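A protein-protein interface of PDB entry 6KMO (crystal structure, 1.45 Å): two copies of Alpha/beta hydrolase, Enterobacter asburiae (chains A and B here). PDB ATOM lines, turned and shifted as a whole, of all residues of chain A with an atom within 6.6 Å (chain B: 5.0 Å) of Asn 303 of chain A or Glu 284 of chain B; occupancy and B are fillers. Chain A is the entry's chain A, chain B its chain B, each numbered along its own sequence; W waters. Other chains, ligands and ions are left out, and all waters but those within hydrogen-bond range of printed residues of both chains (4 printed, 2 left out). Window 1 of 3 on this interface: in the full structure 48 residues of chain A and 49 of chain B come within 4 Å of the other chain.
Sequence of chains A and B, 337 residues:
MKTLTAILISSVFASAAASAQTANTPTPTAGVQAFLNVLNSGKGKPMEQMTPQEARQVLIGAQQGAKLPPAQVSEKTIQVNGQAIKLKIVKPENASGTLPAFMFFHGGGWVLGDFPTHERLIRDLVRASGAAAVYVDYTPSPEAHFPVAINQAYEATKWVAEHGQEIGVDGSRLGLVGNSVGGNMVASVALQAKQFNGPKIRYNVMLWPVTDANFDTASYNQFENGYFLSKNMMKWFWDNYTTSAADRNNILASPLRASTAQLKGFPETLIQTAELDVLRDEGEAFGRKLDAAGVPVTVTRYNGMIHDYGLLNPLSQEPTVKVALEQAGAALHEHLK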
ATOM      1  N   ASN A  24      -1.414  23.526  24.776  1.00  0.00           N
ATOM      2  CA  ASN A  24      -0.880  23.077  23.483  1.00  0.00           C
ATOM      3  C   ASN A  24      -1.899  23.351  22.372  1.00  0.00           C
ATOM      4  O   ASN A  24      -2.484  22.454  21.761  1.00  0.00           O
ATOM      5  CB  ASN A  24      -0.478  21.606  23.583  1.00  0.00           C
ATOM      6  CG  ASN A  24       0.159  21.077  22.308  1.00  0.00           C
ATOM      7  OD1 ASN A  24       0.880  21.794  21.607  1.00  0.00           O
ATOM      8  ND2 ASN A  24      -0.097  19.795  22.011  1.00  0.00           N
ATOM      9  N   THR A  27      -1.239  26.293  16.392  1.00  0.00           N
ATOM     10  CA  THR A  27      -0.862  27.549  15.759  1.00  0.00           C
ATOM     11  C   THR A  27       0.076  27.242  14.604  1.00  0.00           C
ATOM     12  O   THR A  27       0.823  26.257  14.661  1.00  0.00           O
ATOM     13  CB  THR A  27      -0.154  28.493  16.744  1.00  0.00           C
ATOM     14  OG1 THR A  27       1.124  27.963  17.099  1.00  0.00           O
ATOM     15  CG2 THR A  27      -0.972  28.657  18.006  1.00  0.00           C
ATOM     16  N   PRO A  28       0.043  28.032  13.533  1.00  0.00           N
ATOM     17  CA  PRO A  28       1.008  27.828  12.452  1.00  0.00           C
ATOM     18  C   PRO A  28       2.415  28.126  12.925  1.00  0.00           C
ATOM     19  O   PRO A  28       2.630  28.940  13.823  1.00  0.00           O
ATOM     20  CB  PRO A  28       0.580  28.852  11.393  1.00  0.00           C
ATOM     21  CG  PRO A  28      -0.838  29.207  11.724  1.00  0.00           C
ATOM     22  CD  PRO A  28      -0.892  29.133  13.226  1.00  0.00           C
ATOM     23  N   THR A  29       3.395  27.487  12.295  1.00  0.00           N
ATOM     24  CA  THR A  29       4.760  27.932  12.498  1.00  0.00           C
ATOM     25  C   THR A  29       4.919  29.359  11.971  1.00  0.00           C
ATOM     26  O   THR A  29       4.072  29.880  11.244  1.00  0.00           O
ATOM     27  CB  THR A  29       5.762  27.062  11.757  1.00  0.00           C
ATOM     28  OG1 THR A  29       5.501  27.178  10.357  1.00  0.00           O
ATOM     29  CG2 THR A  29       5.699  25.623  12.209  1.00  0.00           C
ATOM     30  N   THR A 273      -0.652  13.884   8.120  1.00  0.00           N
ATOM     31  CA  THR A 273      -1.664  14.922   8.252  1.00  0.00           C
ATOM     32  C   THR A 273      -1.015  16.225   8.706  1.00  0.00           C
ATOM     33  O   THR A 273       0.069  16.245   9.292  1.00  0.00           O
ATOM     34  CB  THR A 273      -2.780  14.514   9.215  1.00  0.00           C
ATOM     35  OG1 THR A 273      -2.193  14.320  10.500  1.00  0.00           O
ATOM     36  CG2 THR A 273      -3.519  13.271   8.729  1.00  0.00           C
ATOM     37  N   ALA A 274      -1.703  17.319   8.400  1.00  0.00           N
ATOM     38  CA  ALA A 274      -1.314  18.653   8.835  1.00  0.00           C
ATOM     39  C   ALA A 274      -2.156  19.055  10.030  1.00  0.00           C
ATOM     40  O   ALA A 274      -3.380  18.872  10.028  1.00  0.00           O
ATOM     41  CB  ALA A 274      -1.538  19.654   7.708  1.00  0.00           C
ATOM     42  N   GLU A 275      -1.513  19.637  11.051  1.00  0.00           N
ATOM     43  CA  GLU A 275      -2.245  19.986  12.270  1.00  0.00           C
ATOM     44  C   GLU A 275      -3.376  20.972  11.995  1.00  0.00           C
ATOM     45  O   GLU A 275      -4.441  20.876  12.610  1.00  0.00           O
ATOM     46  CB  GLU A 275      -1.293  20.551  13.331  1.00  0.00           C
ATOM     47  CG  GLU A 275      -1.989  20.986  14.623  1.00  0.00           C
ATOM     48  CD  GLU A 275      -1.067  21.654  15.614  1.00  0.00           C
ATOM     49  OE1 GLU A 275      -0.047  22.256  15.214  1.00  0.00           O
ATOM     50  OE2 GLU A 275      -1.390  21.557  16.820  1.00  0.00           O
ATOM     51  N   LEU A 276      -3.162  21.939  11.104  1.00  0.00           N
ATOM     52  CA  LEU A 276      -4.134  23.014  10.883  1.00  0.00           C
ATOM     53  C   LEU A 276      -4.758  22.861   9.504  1.00  0.00           C
ATOM     54  O   LEU A 276      -4.582  23.718   8.642  1.00  0.00           O
ATOM     55  CB  LEU A 276      -3.472  24.389  11.069  1.00  0.00           C
ATOM     56  CG  LEU A 276      -2.931  24.630  12.492  1.00  0.00           C
ATOM     57  CD1 LEU A 276      -1.438  24.415  12.537  1.00  0.00           C
ATOM     58  CD2 LEU A 276      -3.291  26.032  12.996  1.00  0.00           C
ATOM     59  N   ARG A 301       1.155  13.163  12.295  1.00  0.00           N
ATOM     60  CA  ARG A 301       0.680  14.537  12.229  1.00  0.00           C
ATOM     61  C   ARG A 301       1.871  15.479  12.340  1.00  0.00           C
ATOM     62  O   ARG A 301       2.658  15.379  13.284  1.00  0.00           O
ATOM     63  CB  ARG A 301      -0.293  14.817  13.376  1.00  0.00           C
ATOM     64  CG  ARG A 301      -0.822  16.242  13.419  1.00  0.00           C
ATOM     65  CD  ARG A 301      -1.530  16.556  14.720  1.00  0.00           C
ATOM     66  NE  ARG A 301      -2.826  15.906  14.792  1.00  0.00           N
ATOM     67  CZ  ARG A 301      -3.797  16.249  15.622  1.00  0.00           C
ATOM     68  NH1 ARG A 301      -3.600  17.222  16.492  1.00  0.00           N
ATOM     69  NH2 ARG A 301      -4.957  15.615  15.583  1.00  0.00           N
ATOM     70  N   TYR A 302       2.004  16.392  11.384  1.00  0.00           N
ATOM     71  CA  TYR A 302       3.059  17.401  11.386  1.00  0.00           C
ATOM     72  C   TYR A 302       2.481  18.692  11.957  1.00  0.00           C
ATOM     73  O   TYR A 302       1.557  19.284  11.381  1.00  0.00           O
ATOM     74  CB  TYR A 302       3.670  17.581   9.988  1.00  0.00           C
ATOM     75  CG  TYR A 302       4.549  16.395   9.613  1.00  0.00           C
ATOM     76  CD1 TYR A 302       3.989  15.229   9.130  1.00  0.00           C
ATOM     77  CD2 TYR A 302       5.917  16.429   9.803  1.00  0.00           C
ATOM     78  CE1 TYR A 302       4.771  14.128   8.825  1.00  0.00           C
ATOM     79  CE2 TYR A 302       6.714  15.328   9.491  1.00  0.00           C
ATOM     80  CZ  TYR A 302       6.124  14.187   9.000  1.00  0.00           C
ATOM     81  OH  TYR A 302       6.870  13.062   8.688  1.00  0.00           O
ATOM     82  N   ASN A 303       2.998  19.105  13.110  1.00  0.00           N
ATOM     83  CA  ASN A 303       2.429  20.270  13.770  1.00  0.00           C
ATOM     84  C   ASN A 303       2.821  21.581  13.087  1.00  0.00           C
ATOM     85  O   ASN A 303       3.851  21.702  12.422  1.00  0.00           O
ATOM     86  CB  ASN A 303       2.818  20.298  15.246  1.00  0.00           C
ATOM     87  CG  ASN A 303       1.862  19.544  16.124  1.00  0.00           C
ATOM     88  OD1 ASN A 303       0.936  18.870  15.659  1.00  0.00           O
ATOM     89  ND2 ASN A 303       2.059  19.665  17.429  1.00  0.00           N
ATOM     90  N   GLY A 304       1.935  22.568  13.222  1.00  0.00           N
ATOM     91  CA  GLY A 304       2.183  23.889  12.715  1.00  0.00           C
ATOM     92  C   GLY A 304       1.932  24.046  11.236  1.00  0.00           C
ATOM     93  O   GLY A 304       2.146  25.142  10.702  1.00  0.00           O
ATOM     94  N   MET A 305       1.496  22.987  10.560  1.00  0.00           N
ATOM     95  CA  MET A 305       1.369  22.974   9.110  1.00  0.00           C
ATOM     96  C   MET A 305      -0.078  23.183   8.680  1.00  0.00           C
ATOM     97  O   MET A 305      -1.029  22.791   9.366  1.00  0.00           O
ATOM     98  CB  MET A 305       1.862  21.637   8.524  1.00  0.00           C
ATOM     99  CG  MET A 305       3.346  21.365   8.641  1.00  0.00           C
ATOM    100  SD  MET A 305       4.445  22.638   7.821  1.00  0.00           S
ATOM    101  CE  MET A 305       4.953  23.623   9.310  1.00  0.00           C
ATOM    102  N   THR A 320       9.936  21.983   8.483  1.00  0.00           N
ATOM    103  CA  THR A 320       9.065  20.820   8.603  1.00  0.00           C
ATOM    104  C   THR A 320       8.801  20.179   7.251  1.00  0.00           C
ATOM    105  O   THR A 320       8.673  18.957   7.160  1.00  0.00           O
ATOM    106  CB  THR A 320       7.742  21.230   9.244  1.00  0.00           C
ATOM    107  OG1 THR A 320       7.963  21.627  10.592  1.00  0.00           O
ATOM    108  CG2 THR A 320       6.708  20.103   9.242  1.00  0.00           C
ATOM    109  N   THR B 273       6.552  13.000  19.126  1.00  0.00           N
ATOM    110  CA  THR B 273       5.705  12.753  20.278  1.00  0.00           C
ATOM    111  C   THR B 273       4.773  11.578  20.014  1.00  0.00           C
ATOM    112  O   THR B 273       4.508  11.200  18.857  1.00  0.00           O
ATOM    113  CB  THR B 273       4.877  13.980  20.647  1.00  0.00           C
ATOM    114  OG1 THR B 273       4.037  14.284  19.541  1.00  0.00           O
ATOM    115  CG2 THR B 273       5.749  15.164  21.009  1.00  0.00           C
ATOM    116  N   ARG B 280       3.129  14.191  25.919  1.00  0.00           N
ATOM    117  CA  ARG B 280       2.934  14.678  24.561  1.00  0.00           C
ATOM    118  C   ARG B 280       2.857  16.201  24.499  1.00  0.00           C
ATOM    119  O   ARG B 280       3.532  16.840  23.678  1.00  0.00           O
ATOM    120  CB  ARG B 280       1.646  14.084  24.007  1.00  0.00           C
ATOM    121  CG  ARG B 280       1.287  14.524  22.604  1.00  0.00           C
ATOM    122  CD  ARG B 280      -0.131  14.167  22.315  1.00  0.00           C
ATOM    123  NE  ARG B 280      -1.053  15.067  23.006  1.00  0.00           N
ATOM    124  CZ  ARG B 280      -2.356  14.875  23.099  1.00  0.00           C
ATOM    125  NH1 ARG B 280      -2.919  13.769  22.640  1.00  0.00           N
ATOM    126  NH2 ARG B 280      -3.115  15.794  23.686  1.00  0.00           N
ATOM    127  N   ASP B 281       2.004  16.801  25.332  1.00  0.00           N
ATOM    128  CA  ASP B 281       1.723  18.224  25.176  1.00  0.00           C
ATOM    129  C   ASP B 281       2.956  19.073  25.474  1.00  0.00           C
ATOM    130  O   ASP B 281       3.215  20.051  24.777  1.00  0.00           O
ATOM    131  CB  ASP B 281       0.544  18.644  26.050  1.00  0.00           C
ATOM    132  CG  ASP B 281      -0.792  18.234  25.491  1.00  0.00           C
ATOM    133  OD1 ASP B 281      -0.869  17.685  24.366  1.00  0.00           O
ATOM    134  OD2 ASP B 281      -1.791  18.491  26.206  1.00  0.00           O
ATOM    135  N   GLU B 282       3.740  18.715  26.491  1.00  0.00           N
ATOM    136  CA  GLU B 282       4.930  19.510  26.783  1.00  0.00           C
ATOM    137  C   GLU B 282       5.993  19.365  25.708  1.00  0.00           C
ATOM    138  O   GLU B 282       6.790  20.293  25.486  1.00  0.00           O
ATOM    139  CB  GLU B 282       5.497  19.136  28.154  1.00  0.00           C
ATOM    140  CG  GLU B 282       6.204  17.795  28.254  1.00  0.00           C
ATOM    141  CD  GLU B 282       6.316  17.325  29.691  1.00  0.00           C
ATOM    142  OE1 GLU B 282       5.259  17.166  30.341  1.00  0.00           O
ATOM    143  OE2 GLU B 282       7.444  17.117  30.184  1.00  0.00           O
ATOM    144  N   GLY B 283       6.050  18.213  25.040  1.00  0.00           N
ATOM    145  CA  GLY B 283       6.981  18.073  23.935  1.00  0.00           C
ATOM    146  C   GLY B 283       6.572  18.923  22.747  1.00  0.00           C
ATOM    147  O   GLY B 283       7.393  19.619  22.145  1.00  0.00           O
ATOM    148  N   GLU B 284       5.282  18.884  22.393  1.00  0.00           N
ATOM    149  CA  GLU B 284       4.777  19.702  21.294  1.00  0.00           C
ATOM    150  C   GLU B 284       4.883  21.192  21.621  1.00  0.00           C
ATOM    151  O   GLU B 284       5.276  22.000  20.766  1.00  0.00           O
ATOM    152  CB  GLU B 284       3.343  19.283  20.939  1.00  0.00           C
ATOM    153  CG  GLU B 284       3.305  17.842  20.459  1.00  0.00           C
ATOM    154  CD  GLU B 284       1.971  17.338  19.975  1.00  0.00           C
ATOM    155  OE1 GLU B 284       0.990  18.115  19.891  1.00  0.00           O
ATOM    156  OE2 GLU B 284       1.915  16.125  19.672  1.00  0.00           O
ATOM    157  N   ALA B 285       4.575  21.560  22.865  1.00  0.00           N
ATOM    158  CA  ALA B 285       4.688  22.961  23.251  1.00  0.00           C
ATOM    159  C   ALA B 285       6.133  23.440  23.155  1.00  0.00           C
ATOM    160  O   ALA B 285       6.393  24.581  22.761  1.00  0.00           O
ATOM    161  CB  ALA B 285       4.146  23.153  24.662  1.00  0.00           C
ATOM    162  N   PHE B 286       7.094  22.595  23.529  1.00  0.00           N
ATOM    163  CA  PHE B 286       8.486  22.999  23.421  1.00  0.00           C
ATOM    164  C   PHE B 286       8.852  23.265  21.969  1.00  0.00           C
ATOM    165  O   PHE B 286       9.558  24.220  21.664  1.00  0.00           O
ATOM    166  CB  PHE B 286       9.397  21.946  24.034  1.00  0.00           C
ATOM    167  CG  PHE B 286      10.843  22.361  24.079  1.00  0.00           C
ATOM    168  CD1 PHE B 286      11.241  23.467  24.815  1.00  0.00           C
ATOM    169  CD2 PHE B 286      11.804  21.665  23.375  1.00  0.00           C
ATOM    170  CE1 PHE B 286      12.570  23.862  24.845  1.00  0.00           C
ATOM    171  CE2 PHE B 286      13.135  22.055  23.409  1.00  0.00           C
ATOM    172  CZ  PHE B 286      13.511  23.161  24.151  1.00  0.00           C
ATOM    173  N   GLY B 287       8.349  22.436  21.047  1.00  0.00           N
ATOM    174  CA  GLY B 287       8.609  22.676  19.644  1.00  0.00           C
ATOM    175  C   GLY B 287       8.081  24.018  19.165  1.00  0.00           C
ATOM    176  O   GLY B 287       8.738  24.707  18.378  1.00  0.00           O
ATOM    177  N   ARG B 288       6.890  24.401  19.625  1.00  0.00           N
ATOM    178  CA  ARG B 288       6.349  25.705  19.260  1.00  0.00           C
ATOM    179  C   ARG B 288       7.221  26.838  19.784  1.00  0.00           C
ATOM    180  O   ARG B 288       7.449  27.822  19.078  1.00  0.00           O
ATOM    181  CB  ARG B 288       4.917  25.855  19.768  1.00  0.00           C
ATOM    182  CG  ARG B 288       3.971  24.773  19.275  1.00  0.00           C
ATOM    183  CD  ARG B 288       2.506  25.134  19.525  1.00  0.00           C
ATOM    184  NE  ARG B 288       1.633  23.973  19.598  1.00  0.00           N
ATOM    185  CZ  ARG B 288       1.018  23.395  18.581  1.00  0.00           C
ATOM    186  NH1 ARG B 288       1.172  23.852  17.330  1.00  0.00           N
ATOM    187  NH2 ARG B 288       0.240  22.349  18.837  1.00  0.00           N
ATOM    188  N   VAL B 299       8.034  19.021  14.363  1.00  0.00           N
ATOM    189  CA  VAL B 299       7.332  18.288  15.414  1.00  0.00           C
ATOM    190  C   VAL B 299       6.386  17.294  14.752  1.00  0.00           C
ATOM    191  O   VAL B 299       5.474  17.696  14.013  1.00  0.00           O
ATOM    192  CB  VAL B 299       6.560  19.221  16.354  1.00  0.00           C
ATOM    193  CG1 VAL B 299       5.839  18.417  17.441  1.00  0.00           C
ATOM    194  CG2 VAL B 299       7.490  20.241  16.984  1.00  0.00           C
ATOM    195  N   ARG B 301       3.832  14.091  15.564  1.00  0.00           N
ATOM    196  CA  ARG B 301       3.077  13.251  16.476  1.00  0.00           C
ATOM    197  C   ARG B 301       2.751  11.939  15.771  1.00  0.00           C
ATOM    198  O   ARG B 301       2.170  11.950  14.679  1.00  0.00           O
ATOM    199  CB  ARG B 301       1.773  13.947  16.893  1.00  0.00           C
ATOM    200  CG  ARG B 301       0.871  13.129  17.811  1.00  0.00           C
ATOM    201  CD  ARG B 301      -0.518  13.721  17.936  1.00  0.00           C
ATOM    202  NE  ARG B 301      -0.499  14.932  18.720  1.00  0.00           N
ATOM    203  CZ  ARG B 301      -1.579  15.504  19.231  1.00  0.00           C
ATOM    204  NH1 ARG B 301      -2.775  14.990  18.979  1.00  0.00           N
ATOM    205  NH2 ARG B 301      -1.443  16.581  19.993  1.00  0.00           N
HETATM  206  O   HOH W   1       6.422  20.818  12.715  1.00  0.00           O
HETATM  207  O   HOH W   2      -3.577  13.075  16.951  1.00  0.00           O
HETATM  208  O   HOH W   3       3.186  25.503  15.902  1.00  0.00           O
HETATM  209  O   HOH W   4       4.257  21.470  18.116  1.00  0.00           O
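Hydrophobic or aromatic side chains of chain B that line the printed part of chain A: Val 299.
Printed residues of chain A that touch a printed residue of chain B: Asn 24, Thr 27, Glu 275, Arg 301, Tyr 302 and Asn 303.
Among the printed residues, 12 pairs touch across the chains.
Among the printed residues, Asp or Glu carboxylates within 4 Å of a Lys or Arg side-chain nitrogen of the other chain: Glu 275 of chain A with Arg 288 of chain B (2.7 Å).
Water W1 lies within hydrogen-bond range of O of Asn 303 of chain A, OG1 of Thr 320 of chain A and N of Val 299 of chain B.
Water W3 lies within hydrogen-bond range of O of Thr 27 of chain A and NH1 of Arg 288 of chain B.
Water W4 bridges the backbone carbonyl oxygen (O) of Glu 284 of chain B (2.9 Å) and the side-chain amide nitrogen (ND2) of Asn 303 of chain A (2.9 Å).
Water W2 lies within hydrogen-bond range of the guanidinium group of Arg 301 of chain B and the guanidinium group of Arg 301 of chain A.
The side-chain amide nitrogen (ND2) of Asn 24 of chain A sits at hydrogen-bond distance from the side-chain carboxylate (OD1) of Asp 281 of chain B, 3.3 Å away.
ND2 of Asn 303 of chain A is in hydrogen-bond range of OE1 of Glu 284 of chain B, 3.1 Å away.
O of Val 299 of chain B is in hydrogen-bond range of N of Asn 303 of chain A (3.0 Å).
The backbone NH (N) of Arg 301 of chain A lies within hydrogen-bond range of the backbone carbonyl oxygen (O) of Arg 301 of chain B (2.9 Å).
The guanidinium group of Arg 288 of chain B sits at hydrogen-bond distance from the side-chain amide oxygen of Asn 24 of chain A (2.9 Å).
The side-chain amide nitrogen (ND2) of Asn 24 of chain A is in hydrogen-bond range of the side-chain carboxylate (OE1) of Glu 284 of chain B.
The side-chain carboxylate (OE2) of Glu 275 of chain A lies within salt-bridge range of the guanidinium group (NH2) of Arg 288 of chain B (2.7 Å).
Ala 285 of chain B touches Asn 24 of chain A.
Arg 288 of chain B touches Thr 27 of chain A.
Arg 301 of chain A touches Val 299 of chain B (O to O, 3.7 Å).
CA of Tyr 302 of chain A touches O of Val 299 of chain B, 3.6 Å away.
Asn 303 of chain A touches Arg 288 of chain B.
Of the printed residues of chain B, Glu 275 of chain A touches Arg 288.
Printed residues of chain B within 4 Å of Arg 301 of chain A: Val 299 (3.7 Å) and Arg 301 (2.9 Å).
Asn 303 of chain A touches just these residues of chain B: Glu 284 (3.1 Å), Arg 288 (3.5 Å) and Val 299 (3.0 Å).
Of the printed residues of chain A, Asp 281 of chain B touches Asn 24.
Gly 283 of chain B touches none of the printed residues of chain A.
Glu 284 of chain B touches just these residues of chain A: Asn 24 (2.9 Å) and Asn 303 (3.1 Å).
Of the printed residues of chain A, Ala 285 of chain B touches Asn 24 (3.9 Å).
Arg 301 of chain B touches its own counterpart, Arg 301 of chain A.
2 positions are printed for both chains.
Of the 12 pairs that touch across the chains among the printed residues, 1 has its exchanged pair printed and touching as well.
The guanidinium group of Arg 280 of chain B is in salt-bridge range of the side-chain carboxylate of Asp 281 of chain B (3.0 Å).
The backbone NH of Gly 304 of chain A is in hydrogen-bond range of the side-chain carboxylate of Glu 275 of chain A (2.8 Å).
O of Tyr 302 of chain A sits at hydrogen-bond distance from N of Glu 275 of chain A, 3.1 Å away.
The side-chain carboxylate (OE2) of Glu 284 of chain B lies within salt-bridge range of the guanidinium group (NE) of Arg 301 of chain B.
OG1 of Thr 273 of chain B sits at hydrogen-bond distance from OE2 of Glu 284 of chain B (2.8 Å).
N of Tyr 302 of chain A sits at hydrogen-bond distance from O of Thr 273 of chain A (2.9 Å).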
